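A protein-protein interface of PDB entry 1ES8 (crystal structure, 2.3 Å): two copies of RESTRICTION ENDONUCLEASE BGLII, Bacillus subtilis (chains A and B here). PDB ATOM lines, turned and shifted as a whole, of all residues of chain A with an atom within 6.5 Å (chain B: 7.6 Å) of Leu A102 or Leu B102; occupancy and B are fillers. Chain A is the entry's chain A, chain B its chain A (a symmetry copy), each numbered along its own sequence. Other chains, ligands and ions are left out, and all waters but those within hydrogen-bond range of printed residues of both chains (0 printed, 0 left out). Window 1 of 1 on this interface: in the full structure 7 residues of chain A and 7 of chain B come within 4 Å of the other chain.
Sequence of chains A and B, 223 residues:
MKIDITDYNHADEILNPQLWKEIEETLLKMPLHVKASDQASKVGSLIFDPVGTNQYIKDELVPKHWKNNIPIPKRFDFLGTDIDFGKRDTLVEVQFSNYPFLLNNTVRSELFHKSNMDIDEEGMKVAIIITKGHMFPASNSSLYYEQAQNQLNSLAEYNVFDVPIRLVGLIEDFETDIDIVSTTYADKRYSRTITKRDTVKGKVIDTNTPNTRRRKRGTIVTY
OG1 of Thr A106 lies within hydrogen-bond range of O of Leu A102, at 3.0 Å. The backbone carbonyl oxygen (O) of Leu B102 is in hydrogen-bond range of the side-chain hydroxyl (OG1) of Thr B106, 3.0 Å away. OG of Ser B154 sits at hydrogen-bond distance from O of Asn B150, at 3.2 Å.
Ser B154 touches Pro A100 (CB to CB, 3.96 Å). Leu A102 touches Leu B102.
Of chain A, only Leu A102 (3.6 Å) comes within 4 Å of Leu B102. Of the printed residues of chain A, Ser B154 touches Pro A100 (3.96 Å). Of the printed residues of chain B, Pro A100 touches Ser B154 (3.96 Å). Val A107 touches none of the printed residues of chain B. Phe B101 touches none of the printed residues of chain A. The nearest residue of chain B that does not touch Leu A102 is Gln B151 (5.0 Å). The nearest printed residue of chain B that does not touch Pro A100 is Leu B155 (6.0 Å).
Printed residues of chain B that touch a printed residue of chain A: Leu B102 and Ser B154. Hydrophobic or aromatic side chains of chain B that line the printed part of chain A: Leu B102. Hydrophobic or aromatic side chains of chain A within 4 Å of the printed part of chain B: Pro A100 and Leu A102. Among the printed residues, 2 pairs touch across the chains.
Leu A102 touches its own counterpart, Leu B102. 13 positions are printed for both chains. Of the 2 pairs that touch across the chains among the printed residues, 1 has its exchanged pair printed and touching as well.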
ATOM      1  N   TYR A  99      15.979  10.572 -10.417  1.00  0.00           N
ATOM      2  CA  TYR A  99      15.494  11.933 -10.302  1.00  0.00           C
ATOM      3  C   TYR A  99      15.814  12.339  -8.855  1.00  0.00           C
ATOM      4  O   TYR A  99      15.658  11.534  -7.937  1.00  0.00           O
ATOM      5  CB  TYR A  99      13.990  11.934 -10.583  1.00  0.00           C
ATOM      6  CG  TYR A  99      13.350  13.293 -10.714  1.00  0.00           C
ATOM      7  CD1 TYR A  99      12.863  13.965  -9.595  1.00  0.00           C
ATOM      8  CD2 TYR A  99      13.210  13.902 -11.961  1.00  0.00           C
ATOM      9  CE1 TYR A  99      12.245  15.216  -9.711  1.00  0.00           C
ATOM     10  CE2 TYR A  99      12.597  15.155 -12.091  1.00  0.00           C
ATOM     11  CZ  TYR A  99      12.115  15.806 -10.958  1.00  0.00           C
ATOM     12  OH  TYR A  99      11.509  17.042 -11.067  1.00  0.00           O
ATOM     13  N   PRO A 100      16.279  13.583  -8.633  1.00  0.00           N
ATOM     14  CA  PRO A 100      16.623  14.063  -7.280  1.00  0.00           C
ATOM     15  C   PRO A 100      15.510  13.843  -6.261  1.00  0.00           C
ATOM     16  O   PRO A 100      14.460  14.482  -6.325  1.00  0.00           O
ATOM     17  CB  PRO A 100      16.947  15.544  -7.506  1.00  0.00           C
ATOM     18  CG  PRO A 100      16.083  15.899  -8.667  1.00  0.00           C
ATOM     19  CD  PRO A 100      16.258  14.707  -9.586  1.00  0.00           C
ATOM     20  N   PHE A 101      15.759  12.942  -5.315  1.00  0.00           N
ATOM     21  CA  PHE A 101      14.777  12.575  -4.295  1.00  0.00           C
ATOM     22  C   PHE A 101      14.088  13.703  -3.527  1.00  0.00           C
ATOM     23  O   PHE A 101      12.875  13.895  -3.652  1.00  0.00           O
ATOM     24  CB  PHE A 101      15.405  11.605  -3.289  1.00  0.00           C
ATOM     25  CG  PHE A 101      14.434  11.088  -2.263  1.00  0.00           C
ATOM     26  CD1 PHE A 101      13.377  10.264  -2.639  1.00  0.00           C
ATOM     27  CD2 PHE A 101      14.553  11.452  -0.929  1.00  0.00           C
ATOM     28  CE1 PHE A 101      12.451   9.812  -1.704  1.00  0.00           C
ATOM     29  CE2 PHE A 101      13.628  11.006   0.018  1.00  0.00           C
ATOM     30  CZ  PHE A 101      12.575  10.184  -0.371  1.00  0.00           C
ATOM     31  N   LEU A 102      14.850  14.433  -2.717  1.00  0.00           N
ATOM     32  CA  LEU A 102      14.275  15.522  -1.927  1.00  0.00           C
ATOM     33  C   LEU A 102      13.557  16.571  -2.772  1.00  0.00           C
ATOM     34  O   LEU A 102      12.443  16.972  -2.449  1.00  0.00           O
ATOM     35  CB  LEU A 102      15.358  16.192  -1.067  1.00  0.00           C
ATOM     36  CG  LEU A 102      15.954  15.309   0.042  1.00  0.00           C
ATOM     37  CD1 LEU A 102      17.058  16.062   0.771  1.00  0.00           C
ATOM     38  CD2 LEU A 102      14.857  14.893   1.022  1.00  0.00           C
ATOM     39  N   LEU A 103      14.192  17.015  -3.850  1.00  0.00           N
ATOM     40  CA  LEU A 103      13.582  18.018  -4.713  1.00  0.00           C
ATOM     41  C   LEU A 103      12.310  17.442  -5.330  1.00  0.00           C
ATOM     42  O   LEU A 103      11.275  18.106  -5.375  1.00  0.00           O
ATOM     43  CB  LEU A 103      14.568  18.438  -5.809  1.00  0.00           C
ATOM     44  CG  LEU A 103      14.253  19.674  -6.667  1.00  0.00           C
ATOM     45  CD1 LEU A 103      13.372  19.299  -7.844  1.00  0.00           C
ATOM     46  CD2 LEU A 103      13.598  20.743  -5.808  1.00  0.00           C
ATOM     47  N   ASN A 104      12.398  16.197  -5.789  1.00  0.00           N
ATOM     48  CA  ASN A 104      11.259  15.502  -6.393  1.00  0.00           C
ATOM     49  C   ASN A 104      10.064  15.483  -5.447  1.00  0.00           C
ATOM     50  O   ASN A 104       8.956  15.878  -5.815  1.00  0.00           O
ATOM     51  CB  ASN A 104      11.632  14.053  -6.720  1.00  0.00           C
ATOM     52  CG  ASN A 104      10.523  13.308  -7.457  1.00  0.00           C
ATOM     53  OD1 ASN A 104      10.432  12.079  -7.383  1.00  0.00           O
ATOM     54  ND2 ASN A 104       9.685  14.046  -8.182  1.00  0.00           N
ATOM     55  N   ASN A 105      10.293  15.020  -4.226  1.00  0.00           N
ATOM     56  CA  ASN A 105       9.216  14.932  -3.253  1.00  0.00           C
ATOM     57  C   ASN A 105       8.789  16.266  -2.646  1.00  0.00           C
ATOM     58  O   ASN A 105       7.639  16.413  -2.230  1.00  0.00           O
ATOM     59  CB  ASN A 105       9.579  13.925  -2.158  1.00  0.00           C
ATOM     60  CG  ASN A 105       9.613  12.495  -2.675  1.00  0.00           C
ATOM     61  OD1 ASN A 105      10.619  12.038  -3.222  1.00  0.00           O
ATOM     62  ND2 ASN A 105       8.505  11.788  -2.518  1.00  0.00           N
ATOM     63  N   THR A 106       9.697  17.237  -2.592  1.00  0.00           N
ATOM     64  CA  THR A 106       9.332  18.544  -2.059  1.00  0.00           C
ATOM     65  C   THR A 106       8.308  19.139  -3.013  1.00  0.00           C
ATOM     66  O   THR A 106       7.330  19.751  -2.592  1.00  0.00           O
ATOM     67  CB  THR A 106      10.544  19.494  -1.973  1.00  0.00           C
ATOM     68  OG1 THR A 106      11.312  19.172  -0.809  1.00  0.00           O
ATOM     69  CG2 THR A 106      10.086  20.955  -1.905  1.00  0.00           C
ATOM     70  N   VAL A 107       8.546  18.944  -4.305  1.00  0.00           N
ATOM     71  CA  VAL A 107       7.653  19.450  -5.337  1.00  0.00           C
ATOM     72  C   VAL A 107       6.322  18.710  -5.281  1.00  0.00           C
ATOM     73  O   VAL A 107       5.257  19.311  -5.445  1.00  0.00           O
ATOM     74  CB  VAL A 107       8.270  19.275  -6.743  1.00  0.00           C
ATOM     75  CG1 VAL A 107       7.245  19.625  -7.808  1.00  0.00           C
ATOM     76  CG2 VAL A 107       9.495  20.163  -6.886  1.00  0.00           C
ATOM     77  N   ALA A 148      16.687   6.854   0.592  1.00  0.00           N
ATOM     78  CA  ALA A 148      15.456   7.620   0.762  1.00  0.00           C
ATOM     79  C   ALA A 148      15.109   7.726   2.240  1.00  0.00           C
ATOM     80  O   ALA A 148      14.628   8.761   2.708  1.00  0.00           O
ATOM     81  CB  ALA A 148      14.307   6.954   0.000  1.00  0.00           C
ATOM     82  N   GLN A 151      17.430  10.226   4.053  1.00  0.00           N
ATOM     83  CA  GLN A 151      16.999  11.592   3.799  1.00  0.00           C
ATOM     84  C   GLN A 151      15.722  11.964   4.541  1.00  0.00           C
ATOM     85  O   GLN A 151      15.626  13.059   5.085  1.00  0.00           O
ATOM     86  CB  GLN A 151      16.855  11.826   2.288  1.00  0.00           C
ATOM     87  CG  GLN A 151      18.181  11.629   1.537  1.00  0.00           C
ATOM     88  CD  GLN A 151      18.128  12.081   0.085  1.00  0.00           C
ATOM     89  OE1 GLN A 151      18.061  13.276  -0.207  1.00  0.00           O
ATOM     90  NE2 GLN A 151      18.158  11.123  -0.834  1.00  0.00           N
ATOM     91  N   LEU A 152      14.750  11.056   4.588  1.00  0.00           N
ATOM     92  CA  LEU A 152      13.505  11.338   5.301  1.00  0.00           C
ATOM     93  C   LEU A 152      13.764  11.336   6.807  1.00  0.00           C
ATOM     94  O   LEU A 152      13.206  12.152   7.529  1.00  0.00           O
ATOM     95  CB  LEU A 152      12.421  10.316   4.934  1.00  0.00           C
ATOM     96  CG  LEU A 152      11.934  10.371   3.476  1.00  0.00           C
ATOM     97  CD1 LEU A 152      10.865   9.305   3.243  1.00  0.00           C
ATOM     98  CD2 LEU A 152      11.359  11.755   3.164  1.00  0.00           C
ATOM     99  N   LEU A 155      14.960  14.791   7.556  1.00  0.00           N
ATOM    100  CA  LEU A 155      13.954  15.840   7.581  1.00  0.00           C
ATOM    101  C   LEU A 155      13.034  15.639   8.780  1.00  0.00           C
ATOM    102  O   LEU A 155      12.643  16.604   9.434  1.00  0.00           O
ATOM    103  CB  LEU A 155      13.123  15.837   6.298  1.00  0.00           C
ATOM    104  CG  LEU A 155      13.862  15.987   4.965  1.00  0.00           C
ATOM    105  CD1 LEU A 155      12.842  15.968   3.834  1.00  0.00           C
ATOM    106  CD2 LEU A 155      14.653  17.286   4.949  1.00  0.00           C
ATOM    107  N   GLN B  95      32.185  22.663   5.528  1.00  0.00           N
ATOM    108  CA  GLN B  95      31.227  21.631   5.885  1.00  0.00           C
ATOM    109  C   GLN B  95      31.813  20.226   5.794  1.00  0.00           C
ATOM    110  O   GLN B  95      31.838  19.633   4.712  1.00  0.00           O
ATOM    111  CB  GLN B  95      29.995  21.731   4.964  1.00  0.00           C
ATOM    112  CG  GLN B  95      29.308  23.095   4.959  1.00  0.00           C
ATOM    113  CD  GLN B  95      28.107  23.167   4.008  1.00  0.00           C
ATOM    114  OE1 GLN B  95      27.471  24.211   3.877  1.00  0.00           O
ATOM    115  NE2 GLN B  95      27.798  22.061   3.347  1.00  0.00           N
ATOM    116  N   TYR B  99      25.845  16.528   8.965  1.00  0.00           N
ATOM    117  CA  TYR B  99      24.607  17.272   9.080  1.00  0.00           C
ATOM    118  C   TYR B  99      23.993  17.225   7.673  1.00  0.00           C
ATOM    119  O   TYR B  99      24.710  17.344   6.680  1.00  0.00           O
ATOM    120  CB  TYR B  99      24.941  18.700   9.518  1.00  0.00           C
ATOM    121  CG  TYR B  99      23.762  19.562   9.893  1.00  0.00           C
ATOM    122  CD1 TYR B  99      23.087  20.308   8.929  1.00  0.00           C
ATOM    123  CD2 TYR B  99      23.332  19.649  11.216  1.00  0.00           C
ATOM    124  CE1 TYR B  99      22.008  21.131   9.272  1.00  0.00           C
ATOM    125  CE2 TYR B  99      22.249  20.467  11.573  1.00  0.00           C
ATOM    126  CZ  TYR B  99      21.594  21.205  10.593  1.00  0.00           C
ATOM    127  OH  TYR B  99      20.524  22.015  10.925  1.00  0.00           O
ATOM    128  N   PRO B 100      22.664  17.037   7.567  1.00  0.00           N
ATOM    129  CA  PRO B 100      21.983  16.967   6.259  1.00  0.00           C
ATOM    130  C   PRO B 100      22.314  18.143   5.344  1.00  0.00           C
ATOM    131  O   PRO B 100      21.912  19.278   5.603  1.00  0.00           O
ATOM    132  CB  PRO B 100      20.500  16.903   6.640  1.00  0.00           C
ATOM    133  CG  PRO B 100      20.453  17.659   7.922  1.00  0.00           C
ATOM    134  CD  PRO B 100      21.675  17.145   8.655  1.00  0.00           C
ATOM    135  N   PHE B 101      23.039  17.854   4.268  1.00  0.00           N
ATOM    136  CA  PHE B 101      23.487  18.873   3.320  1.00  0.00           C
ATOM    137  C   PHE B 101      22.447  19.857   2.783  1.00  0.00           C
ATOM    138  O   PHE B 101      22.520  21.057   3.060  1.00  0.00           O
ATOM    139  CB  PHE B 101      24.197  18.210   2.134  1.00  0.00           C
ATOM    140  CG  PHE B 101      24.787  19.192   1.159  1.00  0.00           C
ATOM    141  CD1 PHE B 101      25.844  20.016   1.534  1.00  0.00           C
ATOM    142  CD2 PHE B 101      24.266  19.318  -0.122  1.00  0.00           C
ATOM    143  CE1 PHE B 101      26.372  20.954   0.653  1.00  0.00           C
ATOM    144  CE2 PHE B 101      24.787  20.257  -1.014  1.00  0.00           C
ATOM    145  CZ  PHE B 101      25.843  21.077  -0.625  1.00  0.00           C
ATOM    146  N   LEU B 102      21.495  19.359   1.999  1.00  0.00           N
ATOM    147  CA  LEU B 102      20.468  20.227   1.423  1.00  0.00           C
ATOM    148  C   LEU B 102      19.682  21.013   2.469  1.00  0.00           C
ATOM    149  O   LEU B 102      19.484  22.215   2.321  1.00  0.00           O
ATOM    150  CB  LEU B 102      19.504  19.410   0.547  1.00  0.00           C
ATOM    151  CG  LEU B 102      20.124  18.809  -0.726  1.00  0.00           C
ATOM    152  CD1 LEU B 102      19.090  17.971  -1.464  1.00  0.00           C
ATOM    153  CD2 LEU B 102      20.648  19.925  -1.629  1.00  0.00           C
ATOM    154  N   LEU B 103      19.237  20.338   3.521  1.00  0.00           N
ATOM    155  CA  LEU B 103      18.476  21.009   4.568  1.00  0.00           C
ATOM    156  C   LEU B 103      19.360  22.058   5.237  1.00  0.00           C
ATOM    157  O   LEU B 103      18.929  23.184   5.478  1.00  0.00           O
ATOM    158  CB  LEU B 103      17.984  19.985   5.598  1.00  0.00           C
ATOM    159  CG  LEU B 103      16.937  20.413   6.638  1.00  0.00           C
ATOM    160  CD1 LEU B 103      17.606  21.046   7.843  1.00  0.00           C
ATOM    161  CD2 LEU B 103      15.937  21.365   6.000  1.00  0.00           C
ATOM    162  N   ASN B 104      20.604  21.678   5.517  1.00  0.00           N
ATOM    163  CA  ASN B 104      21.575  22.576   6.144  1.00  0.00           C
ATOM    164  C   ASN B 104      21.736  23.859   5.337  1.00  0.00           C
ATOM    165  O   ASN B 104      21.616  24.964   5.868  1.00  0.00           O
ATOM    166  CB  ASN B 104      22.946  21.897   6.237  1.00  0.00           C
ATOM    167  CG  ASN B 104      23.974  22.741   6.985  1.00  0.00           C
ATOM    168  OD1 ASN B 104      25.180  22.608   6.762  1.00  0.00           O
ATOM    169  ND2 ASN B 104      23.504  23.600   7.886  1.00  0.00           N
ATOM    170  N   ASN B 105      22.010  23.708   4.047  1.00  0.00           N
ATOM    171  CA  ASN B 105      22.210  24.867   3.193  1.00  0.00           C
ATOM    172  C   ASN B 105      20.934  25.613   2.814  1.00  0.00           C
ATOM    173  O   ASN B 105      20.979  26.814   2.544  1.00  0.00           O
ATOM    174  CB  ASN B 105      23.000  24.466   1.943  1.00  0.00           C
ATOM    175  CG  ASN B 105      24.439  24.096   2.262  1.00  0.00           C
ATOM    176  OD1 ASN B 105      24.739  22.959   2.635  1.00  0.00           O
ATOM    177  ND2 ASN B 105      25.337  25.061   2.134  1.00  0.00           N
ATOM    178  N   THR B 106      19.798  24.919   2.790  1.00  0.00           N
ATOM    179  CA  THR B 106      18.543  25.591   2.474  1.00  0.00           C
ATOM    180  C   THR B 106      18.274  26.575   3.600  1.00  0.00           C
ATOM    181  O   THR B 106      17.832  27.697   3.370  1.00  0.00           O
ATOM    182  CB  THR B 106      17.364  24.601   2.384  1.00  0.00           C
ATOM    183  OG1 THR B 106      17.397  23.944   1.112  1.00  0.00           O
ATOM    184  CG2 THR B 106      16.027  25.331   2.555  1.00  0.00           C
ATOM    185  N   VAL B 107      18.554  26.139   4.823  1.00  0.00           N
ATOM    186  CA  VAL B 107      18.352  26.968   6.002  1.00  0.00           C
ATOM    187  C   VAL B 107      19.337  28.132   5.993  1.00  0.00           C
ATOM    188  O   VAL B 107      18.984  29.261   6.346  1.00  0.00           O
ATOM    189  CB  VAL B 107      18.547  26.152   7.299  1.00  0.00           C
ATOM    190  CG1 VAL B 107      18.528  27.077   8.504  1.00  0.00           C
ATOM    191  CG2 VAL B 107      17.449  25.108   7.425  1.00  0.00           C
ATOM    192  N   ARG B 108      20.575  27.848   5.593  1.00  0.00           N
ATOM    193  CA  ARG B 108      21.611  28.872   5.530  1.00  0.00           C
ATOM    194  C   ARG B 108      21.307  29.826   4.386  1.00  0.00           C
ATOM    195  O   ARG B 108      21.608  31.015   4.454  1.00  0.00           O
ATOM    196  CB  ARG B 108      22.979  28.226   5.311  1.00  0.00           C
ATOM    197  CG  ARG B 108      23.555  27.541   6.535  1.00  0.00           C
ATOM    198  CD  ARG B 108      24.694  26.607   6.148  1.00  0.00           C
ATOM    199  NE  ARG B 108      25.345  26.044   7.324  1.00  0.00           N
ATOM    200  CZ  ARG B 108      26.153  26.726   8.131  1.00  0.00           C
ATOM    201  NH1 ARG B 108      26.422  28.001   7.881  1.00  0.00           N
ATOM    202  NH2 ARG B 108      26.677  26.137   9.197  1.00  0.00           N
ATOM    203  N   SER B 109      20.707  29.287   3.332  1.00  0.00           N
ATOM    204  CA  SER B 109      20.351  30.074   2.159  1.00  0.00           C
ATOM    205  C   SER B 109      19.302  31.118   2.536  1.00  0.00           C
ATOM    206  O   SER B 109      19.353  32.262   2.081  1.00  0.00           O
ATOM    207  CB  SER B 109      19.807  29.153   1.063  1.00  0.00           C
ATOM    208  OG  SER B 109      19.664  29.841  -0.165  1.00  0.00           O
ATOM    209  N   GLU B 110      18.355  30.711   3.374  1.00  0.00           N
ATOM    210  CA  GLU B 110      17.288  31.594   3.824  1.00  0.00           C
ATOM    211  C   GLU B 110      17.870  32.839   4.495  1.00  0.00           C
ATOM    212  O   GLU B 110      17.492  33.967   4.171  1.00  0.00           O
ATOM    213  CB  GLU B 110      16.363  30.830   4.779  1.00  0.00           C
ATOM    214  CG  GLU B 110      15.611  29.682   4.100  1.00  0.00           C
ATOM    215  CD  GLU B 110      15.057  28.658   5.079  1.00  0.00           C
ATOM    216  OE1 GLU B 110      14.313  29.050   6.001  1.00  0.00           O
ATOM    217  OE2 GLU B 110      15.365  27.455   4.920  1.00  0.00           O
ATOM    218  N   LEU B 143      29.705  14.461   5.146  1.00  0.00           N
ATOM    219  CA  LEU B 143      29.614  14.996   3.799  1.00  0.00           C
ATOM    220  C   LEU B 143      30.926  14.933   3.025  1.00  0.00           C
ATOM    221  O   LEU B 143      31.999  15.038   3.606  1.00  0.00           O
ATOM    222  CB  LEU B 143      29.150  16.452   3.864  1.00  0.00           C
ATOM    223  CG  LEU B 143      29.072  17.219   2.538  1.00  0.00           C
ATOM    224  CD1 LEU B 143      27.967  16.624   1.658  1.00  0.00           C
ATOM    225  CD2 LEU B 143      28.799  18.684   2.814  1.00  0.00           C
ATOM    226  N   GLN B 147      29.439  14.272  -3.379  1.00  0.00           N
ATOM    227  CA  GLN B 147      28.047  14.195  -2.957  1.00  0.00           C
ATOM    228  C   GLN B 147      27.405  15.582  -2.931  1.00  0.00           C
ATOM    229  O   GLN B 147      26.258  15.754  -3.341  1.00  0.00           O
ATOM    230  CB  GLN B 147      27.980  13.547  -1.568  1.00  0.00           C
ATOM    231  CG  GLN B 147      26.660  13.687  -0.836  1.00  0.00           C
ATOM    232  CD  GLN B 147      26.703  13.036   0.542  1.00  0.00           C
ATOM    233  OE1 GLN B 147      27.686  13.181   1.283  1.00  0.00           O
ATOM    234  NE2 GLN B 147      25.634  12.321   0.897  1.00  0.00           N
ATOM    235  N   ALA B 148      28.147  16.572  -2.448  1.00  0.00           N
ATOM    236  CA  ALA B 148      27.633  17.936  -2.383  1.00  0.00           C
ATOM    237  C   ALA B 148      27.443  18.487  -3.790  1.00  0.00           C
ATOM    238  O   ALA B 148      26.483  19.211  -4.065  1.00  0.00           O
ATOM    239  CB  ALA B 148      28.596  18.829  -1.596  1.00  0.00           C
ATOM    240  N   ASN B 150      26.927  16.681  -6.555  1.00  0.00           N
ATOM    241  CA  ASN B 150      25.808  15.980  -7.170  1.00  0.00           C
ATOM    242  C   ASN B 150      24.513  16.677  -6.790  1.00  0.00           C
ATOM    243  O   ASN B 150      23.683  16.982  -7.644  1.00  0.00           O
ATOM    244  CB  ASN B 150      25.746  14.538  -6.673  1.00  0.00           C
ATOM    245  CG  ASN B 150      24.547  13.786  -7.222  1.00  0.00           C
ATOM    246  OD1 ASN B 150      24.592  13.248  -8.329  1.00  0.00           O
ATOM    247  ND2 ASN B 150      23.460  13.756  -6.455  1.00  0.00           N
ATOM    248  N   GLN B 151      24.345  16.936  -5.499  1.00  0.00           N
ATOM    249  CA  GLN B 151      23.130  17.579  -5.024  1.00  0.00           C
ATOM    250  C   GLN B 151      22.948  18.989  -5.571  1.00  0.00           C
ATOM    251  O   GLN B 151      21.843  19.360  -5.954  1.00  0.00           O
ATOM    252  CB  GLN B 151      23.092  17.567  -3.489  1.00  0.00           C
ATOM    253  CG  GLN B 151      23.095  16.141  -2.916  1.00  0.00           C
ATOM    254  CD  GLN B 151      22.821  16.089  -1.420  1.00  0.00           C
ATOM    255  OE1 GLN B 151      21.703  16.341  -0.969  1.00  0.00           O
ATOM    256  NE2 GLN B 151      23.846  15.760  -0.642  1.00  0.00           N
ATOM    257  N   LEU B 152      24.023  19.771  -5.632  1.00  0.00           N
ATOM    258  CA  LEU B 152      23.926  21.128  -6.166  1.00  0.00           C
ATOM    259  C   LEU B 152      23.715  21.072  -7.677  1.00  0.00           C
ATOM    260  O   LEU B 152      22.957  21.863  -8.224  1.00  0.00           O
ATOM    261  CB  LEU B 152      25.179  21.943  -5.821  1.00  0.00           C
ATOM    262  CG  LEU B 152      25.380  22.238  -4.325  1.00  0.00           C
ATOM    263  CD1 LEU B 152      26.660  23.045  -4.120  1.00  0.00           C
ATOM    264  CD2 LEU B 152      24.183  23.018  -3.776  1.00  0.00           C
ATOM    265  N   SER B 154      22.089  18.983  -9.163  1.00  0.00           N
ATOM    266  CA  SER B 154      20.675  18.670  -9.328  1.00  0.00           C
ATOM    267  C   SER B 154      19.787  19.880  -9.140  1.00  0.00           C
ATOM    268  O   SER B 154      18.886  20.111  -9.935  1.00  0.00           O
ATOM    269  CB  SER B 154      20.243  17.565  -8.368  1.00  0.00           C
ATOM    270  OG  SER B 154      20.756  16.320  -8.803  1.00  0.00           O
ATOM    271  N   LEU B 155      20.030  20.657  -8.094  1.00  0.00           N
ATOM    272  CA  LEU B 155      19.209  21.838  -7.874  1.00  0.00           C
ATOM    273  C   LEU B 155      19.464  22.851  -8.984  1.00  0.00           C
ATOM    274  O   LEU B 155      18.534  23.499  -9.461  1.00  0.00           O
ATOM    275  CB  LEU B 155      19.518  22.478  -6.521  1.00  0.00           C
ATOM    276  CG  LEU B 155      19.364  21.614  -5.267  1.00  0.00           C
ATOM    277  CD1 LEU B 155      19.710  22.455  -4.045  1.00  0.00           C
ATOM    278  CD2 LEU B 155      17.940  21.087  -5.166  1.00  0.00           C
ATOM    279  N   PHE B 161      18.100  27.435  -6.987  1.00  0.00           N
ATOM    280  CA  PHE B 161      18.703  28.523  -6.236  1.00  0.00           C
ATOM    281  C   PHE B 161      19.495  29.434  -7.161  1.00  0.00           C
ATOM    282  O   PHE B 161      19.983  29.001  -8.205  1.00  0.00           O
ATOM    283  CB  PHE B 161      19.618  27.964  -5.144  1.00  0.00           C
ATOM    284  CG  PHE B 161      20.813  27.214  -5.672  1.00  0.00           C
ATOM    285  CD1 PHE B 161      20.674  25.936  -6.206  1.00  0.00           C
ATOM    286  CD2 PHE B 161      22.075  27.804  -5.657  1.00  0.00           C
ATOM    287  CE1 PHE B 161      21.778  25.247  -6.720  1.00  0.00           C
ATOM    288  CE2 PHE B 161      23.185  27.132  -6.167  1.00  0.00           C
ATOM    289  CZ  PHE B 161      23.039  25.847  -6.702  1.00  0.00           C
